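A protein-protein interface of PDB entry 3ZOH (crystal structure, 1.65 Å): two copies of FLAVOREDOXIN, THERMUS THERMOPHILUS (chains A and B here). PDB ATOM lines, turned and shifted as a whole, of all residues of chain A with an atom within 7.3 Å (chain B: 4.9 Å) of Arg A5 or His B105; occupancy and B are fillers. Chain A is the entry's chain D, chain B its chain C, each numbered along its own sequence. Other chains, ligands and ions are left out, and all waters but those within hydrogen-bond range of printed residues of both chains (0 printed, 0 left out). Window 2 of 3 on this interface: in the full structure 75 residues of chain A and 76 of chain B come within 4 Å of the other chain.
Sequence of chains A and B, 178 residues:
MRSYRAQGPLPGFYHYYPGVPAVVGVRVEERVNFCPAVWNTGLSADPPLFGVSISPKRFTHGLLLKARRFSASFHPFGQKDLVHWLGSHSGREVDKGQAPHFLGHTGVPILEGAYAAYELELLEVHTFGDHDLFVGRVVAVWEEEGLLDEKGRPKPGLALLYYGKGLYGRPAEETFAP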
ATOM      1  N   ARG A   2     -13.796  18.795  23.812  1.00  0.00           N
ATOM      2  CA  ARG A   2     -15.200  19.187  23.673  1.00  0.00           C
ATOM      3  C   ARG A   2     -15.475  20.608  24.196  1.00  0.00           C
ATOM      4  O   ARG A   2     -14.802  21.068  25.133  1.00  0.00           O
ATOM      5  CB  ARG A   2     -16.068  18.179  24.430  1.00  0.00           C
ATOM      6  CG  ARG A   2     -17.554  18.466  24.403  1.00  0.00           C
ATOM      7  CD  ARG A   2     -18.229  17.981  25.673  1.00  0.00           C
ATOM      8  NE  ARG A   2     -19.656  18.261  25.609  1.00  0.00           N
ATOM      9  CZ  ARG A   2     -20.519  18.115  26.611  1.00  0.00           C
ATOM     10  NH1 ARG A   2     -20.127  17.685  27.802  1.00  0.00           N
ATOM     11  NH2 ARG A   2     -21.793  18.407  26.408  1.00  0.00           N
ATOM     12  N   SER A   3     -16.440  21.300  23.583  1.00  0.00           N
ATOM     13  CA  SER A   3     -16.934  22.582  24.105  1.00  0.00           C
ATOM     14  C   SER A   3     -18.417  22.834  23.834  1.00  0.00           C
ATOM     15  O   SER A   3     -19.003  22.277  22.902  1.00  0.00           O
ATOM     16  CB  SER A   3     -16.099  23.767  23.601  1.00  0.00           C
ATOM     17  OG  SER A   3     -16.630  24.321  22.404  1.00  0.00           O
ATOM     18  N   TYR A   4     -19.023  23.676  24.663  1.00  0.00           N
ATOM     19  CA  TYR A   4     -20.391  24.118  24.430  1.00  0.00           C
ATOM     20  C   TYR A   4     -20.653  25.457  25.076  1.00  0.00           C
ATOM     21  O   TYR A   4     -19.938  25.880  25.995  1.00  0.00           O
ATOM     22  CB  TYR A   4     -21.416  23.079  24.911  1.00  0.00           C
ATOM     23  CG  TYR A   4     -21.367  22.740  26.394  1.00  0.00           C
ATOM     24  CD1 TYR A   4     -20.562  21.699  26.865  1.00  0.00           C
ATOM     25  CD2 TYR A   4     -22.156  23.428  27.310  1.00  0.00           C
ATOM     26  CE1 TYR A   4     -20.530  21.376  28.217  1.00  0.00           C
ATOM     27  CE2 TYR A   4     -22.134  23.115  28.658  1.00  0.00           C
ATOM     28  CZ  TYR A   4     -21.323  22.089  29.103  1.00  0.00           C
ATOM     29  OH  TYR A   4     -21.299  21.791  30.439  1.00  0.00           O
ATOM     30  N   ARG A   5     -21.677  26.127  24.571  1.00  0.00           N
ATOM     31  CA  ARG A   5     -22.137  27.377  25.117  1.00  0.00           C
ATOM     32  C   ARG A   5     -23.078  27.047  26.259  1.00  0.00           C
ATOM     33  O   ARG A   5     -23.838  26.082  26.178  1.00  0.00           O
ATOM     34  CB  ARG A   5     -22.857  28.185  24.030  1.00  0.00           C
ATOM     35  CG  ARG A   5     -21.982  29.121  23.181  1.00  0.00           C
ATOM     36  CD  ARG A   5     -20.531  28.691  22.960  1.00  0.00           C
ATOM     37  NE  ARG A   5     -20.368  27.338  22.411  1.00  0.00           N
ATOM     38  CZ  ARG A   5     -20.311  27.028  21.117  1.00  0.00           C
ATOM     39  NH1 ARG A   5     -20.412  27.970  20.186  1.00  0.00           N
ATOM     40  NH2 ARG A   5     -20.150  25.761  20.751  1.00  0.00           N
ATOM     41  N   ALA A   6     -23.012  27.836  27.326  1.00  0.00           N
ATOM     42  CA  ALA A   6     -23.932  27.678  28.446  1.00  0.00           C
ATOM     43  C   ALA A   6     -25.325  28.185  28.073  1.00  0.00           C
ATOM     44  O   ALA A   6     -25.475  29.254  27.457  1.00  0.00           O
ATOM     45  CB  ALA A   6     -23.398  28.379  29.691  1.00  0.00           C
ATOM     46  N   GLN A   7     -26.332  27.392  28.431  1.00  0.00           N
ATOM     47  CA  GLN A   7     -27.723  27.660  28.077  1.00  0.00           C
ATOM     48  C   GLN A   7     -28.622  27.585  29.317  1.00  0.00           C
ATOM     49  O   GLN A   7     -29.845  27.487  29.205  1.00  0.00           O
ATOM     50  CB  GLN A   7     -28.180  26.656  27.007  1.00  0.00           C
ATOM     51  CG  GLN A   7     -27.308  26.654  25.758  1.00  0.00           C
ATOM     52  CD  GLN A   7     -27.168  25.280  25.123  1.00  0.00           C
ATOM     53  OE1 GLN A   7     -28.158  24.618  24.809  1.00  0.00           O
ATOM     54  NE2 GLN A   7     -25.928  24.851  24.919  1.00  0.00           N
ATOM     55  N   GLY A   8     -27.999  27.641  30.494  1.00  0.00           N
ATOM     56  CA  GLY A   8     -28.703  27.591  31.768  1.00  0.00           C
ATOM     57  C   GLY A   8     -27.769  26.903  32.741  1.00  0.00           C
ATOM     58  O   GLY A   8     -26.558  26.938  32.546  1.00  0.00           O
ATOM     59  N   LEU A  10     -25.486  24.115  34.222  1.00  0.00           N
ATOM     60  CA  LEU A  10     -24.675  23.125  33.519  1.00  0.00           C
ATOM     61  C   LEU A  10     -25.115  21.692  33.829  1.00  0.00           C
ATOM     62  O   LEU A  10     -25.639  21.424  34.913  1.00  0.00           O
ATOM     63  CB  LEU A  10     -23.184  23.319  33.839  1.00  0.00           C
ATOM     64  CG  LEU A  10     -22.595  24.732  33.763  1.00  0.00           C
ATOM     65  CD1 LEU A  10     -21.081  24.684  33.947  1.00  0.00           C
ATOM     66  CD2 LEU A  10     -22.960  25.438  32.461  1.00  0.00           C
ATOM     67  N   LEU B 103      -7.575  30.538  22.048  1.00  0.00           N
ATOM     68  CA  LEU B 103      -8.668  31.442  22.307  1.00  0.00           C
ATOM     69  C   LEU B 103      -9.986  30.696  22.283  1.00  0.00           C
ATOM     70  O   LEU B 103     -10.241  29.907  21.374  1.00  0.00           O
ATOM     71  CB  LEU B 103      -8.674  32.577  21.298  1.00  0.00           C
ATOM     72  CG  LEU B 103      -7.468  33.512  21.314  1.00  0.00           C
ATOM     73  CD1 LEU B 103      -7.698  34.565  20.245  1.00  0.00           C
ATOM     74  CD2 LEU B 103      -7.244  34.144  22.688  1.00  0.00           C
ATOM     75  N   GLY B 104     -10.820  30.941  23.295  1.00  0.00           N
ATOM     76  CA  GLY B 104     -12.153  30.326  23.359  1.00  0.00           C
ATOM     77  C   GLY B 104     -13.155  31.008  22.443  1.00  0.00           C
ATOM     78  O   GLY B 104     -12.788  31.851  21.618  1.00  0.00           O
ATOM     79  N   HIS B 105     -14.425  30.651  22.594  1.00  0.00           N
ATOM     80  CA  HIS B 105     -15.499  31.248  21.796  1.00  0.00           C
ATOM     81  C   HIS B 105     -15.646  32.756  21.999  1.00  0.00           C
ATOM     82  O   HIS B 105     -15.903  33.495  21.044  1.00  0.00           O
ATOM     83  CB  HIS B 105     -16.817  30.537  22.085  1.00  0.00           C
ATOM     84  CG  HIS B 105     -16.765  29.066  21.821  1.00  0.00           C
ATOM     85  ND1 HIS B 105     -16.900  28.534  20.556  1.00  0.00           N
ATOM     86  CD2 HIS B 105     -16.563  28.017  22.652  1.00  0.00           C
ATOM     87  CE1 HIS B 105     -16.795  27.218  20.621  1.00  0.00           C
ATOM     88  NE2 HIS B 105     -16.598  26.879  21.883  1.00  0.00           N
ATOM     89  N   THR B 106     -15.458  33.206  23.236  1.00  0.00           N
ATOM     90  CA  THR B 106     -15.595  34.613  23.585  1.00  0.00           C
ATOM     91  C   THR B 106     -14.256  35.340  23.451  1.00  0.00           C
ATOM     92  O   THR B 106     -14.167  36.530  23.746  1.00  0.00           O
ATOM     93  CB  THR B 106     -16.138  34.817  25.025  1.00  0.00           C
ATOM     94  OG1 THR B 106     -15.175  34.353  25.979  1.00  0.00           O
ATOM     95  CG2 THR B 106     -17.459  34.079  25.234  1.00  0.00           C
ATOM     96  N   GLY B 107     -13.228  34.615  23.013  1.00  0.00           N
ATOM     97  CA  GLY B 107     -11.908  35.193  22.746  1.00  0.00           C
ATOM     98  C   GLY B 107     -10.995  35.239  23.956  1.00  0.00           C
ATOM     99  O   GLY B 107      -9.892  35.782  23.894  1.00  0.00           O
ATOM    100  N   GLU B 119     -15.187  29.681  30.150  1.00  0.00           N
ATOM    101  CA  GLU B 119     -15.160  31.055  29.688  1.00  0.00           C
ATOM    102  C   GLU B 119     -16.176  31.838  30.497  1.00  0.00           C
ATOM    103  O   GLU B 119     -17.328  31.404  30.663  1.00  0.00           O
ATOM    104  CB  GLU B 119     -15.497  31.146  28.201  1.00  0.00           C
ATOM    105  CG  GLU B 119     -14.724  30.150  27.368  1.00  0.00           C
ATOM    106  CD  GLU B 119     -14.840  30.414  25.886  1.00  0.00           C
ATOM    107  OE1 GLU B 119     -15.068  31.579  25.506  1.00  0.00           O
ATOM    108  OE2 GLU B 119     -14.672  29.444  25.122  1.00  0.00           O
ATOM    109  N   VAL B 139     -20.163  31.263  30.565  1.00  0.00           N
ATOM    110  CA  VAL B 139     -20.867  31.410  29.290  1.00  0.00           C
ATOM    111  C   VAL B 139     -20.483  30.337  28.275  1.00  0.00           C
ATOM    112  O   VAL B 139     -21.181  30.137  27.270  1.00  0.00           O
ATOM    113  CB  VAL B 139     -20.705  32.823  28.683  1.00  0.00           C
ATOM    114  CG1 VAL B 139     -21.382  33.864  29.562  1.00  0.00           C
ATOM    115  CG2 VAL B 139     -19.246  33.168  28.445  1.00  0.00           C
ATOM    116  N   ALA B 140     -19.366  29.657  28.528  1.00  0.00           N
ATOM    117  CA  ALA B 140     -18.976  28.494  27.731  1.00  0.00           C
ATOM    118  C   ALA B 140     -18.102  27.539  28.524  1.00  0.00           C
ATOM    119  O   ALA B 140     -17.394  27.947  29.448  1.00  0.00           O
ATOM    120  CB  ALA B 140     -18.289  28.912  26.430  1.00  0.00           C
ATOM    121  N   TRP B 142     -15.409  24.074  28.314  1.00  0.00           N
ATOM    122  CA  TRP B 142     -14.501  23.162  27.638  1.00  0.00           C
ATOM    123  C   TRP B 142     -14.267  21.958  28.539  1.00  0.00           C
ATOM    124  O   TRP B 142     -14.064  22.105  29.746  1.00  0.00           O
ATOM    125  CB  TRP B 142     -13.176  23.882  27.302  1.00  0.00           C
ATOM    126  CG  TRP B 142     -13.398  25.001  26.334  1.00  0.00           C
ATOM    127  CD1 TRP B 142     -13.953  26.220  26.605  1.00  0.00           C
ATOM    128  CD2 TRP B 142     -13.127  24.990  24.927  1.00  0.00           C
ATOM    129  NE1 TRP B 142     -14.029  26.972  25.459  1.00  0.00           N
ATOM    130  CE2 TRP B 142     -13.545  26.235  24.410  1.00  0.00           C
ATOM    131  CE3 TRP B 142     -12.590  24.037  24.047  1.00  0.00           C
ATOM    132  CZ2 TRP B 142     -13.410  26.575  23.054  1.00  0.00           C
ATOM    133  CZ3 TRP B 142     -12.464  24.372  22.697  1.00  0.00           C
ATOM    134  CH2 TRP B 142     -12.876  25.626  22.217  1.00  0.00           C
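The side-chain hydroxyl of Ser A3 is in hydrogen-bond range of a ring nitrogen (NE2) of His B105, 2.6 Å away.
O of Val B139 lies within hydrogen-bond range of N of Ala A6 (2.9 Å).
The backbone carbonyl oxygen (O) of Glu B119 lies within hydrogen-bond range of the backbone NH (N) of Val B139, at 2.8 Å.
The backbone carbonyl oxygen of Arg A5 is in hydrogen-bond range of the side-chain amide nitrogen of Gln A7, 2.7 Å away.
OE2 of Glu B119 is in hydrogen-bond range of NE1 of Trp B142, at 2.6 Å.
The backbone NH of His B105 is in hydrogen-bond range of the side-chain carboxylate of Glu B119, at 2.8 Å.
The backbone NH of Glu B119 is in hydrogen-bond range of the backbone carbonyl oxygen of Ala B140, at 2.9 Å.
Among the printed residues, pairs that only touch across the chains: Arg A2 with Trp B142, Ser A3 with Trp B142, Tyr A4 with Ala B140, Arg A5 with His B105 and Arg A5 with Val B139.
Arg A5 touches just these residues of chain B: His B105 (3.6 Å) and Val B139 (3.6 Å).
His B105 touches just these residues of chain A: Ser A3 and Arg A5.
Printed residues of chain A within 4 Å of Val B139: Arg A5 (3.6 Å) and Ala A6 (2.9 Å).
Of the printed residues of chain B, Ala A6 touches Val B139.
Printed residues of chain A within 4 Å of Ala B140: Tyr A4 (3.3 Å).
Of the printed residues of chain B, Arg A2 touches Trp B142.
The nearest residue of chain A that does not touch His B105 is Tyr A4 (4.9 Å).
The nearest printed residue of chain B that does not touch Tyr A4 is Val B139 (4.6 Å).
Of the 8 printed residues of chain A, 5 touch a printed residue of chain B.
Of the 9 printed residues of chain B, 4 touch a printed residue of chain A.
Among the printed residues, 7 pairs touch across the chains.
Among the printed residues, no Asp or Glu carboxylate lies within 4 Å of a Lys or Arg side-chain nitrogen of the other chain.
No position is printed for both chains.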
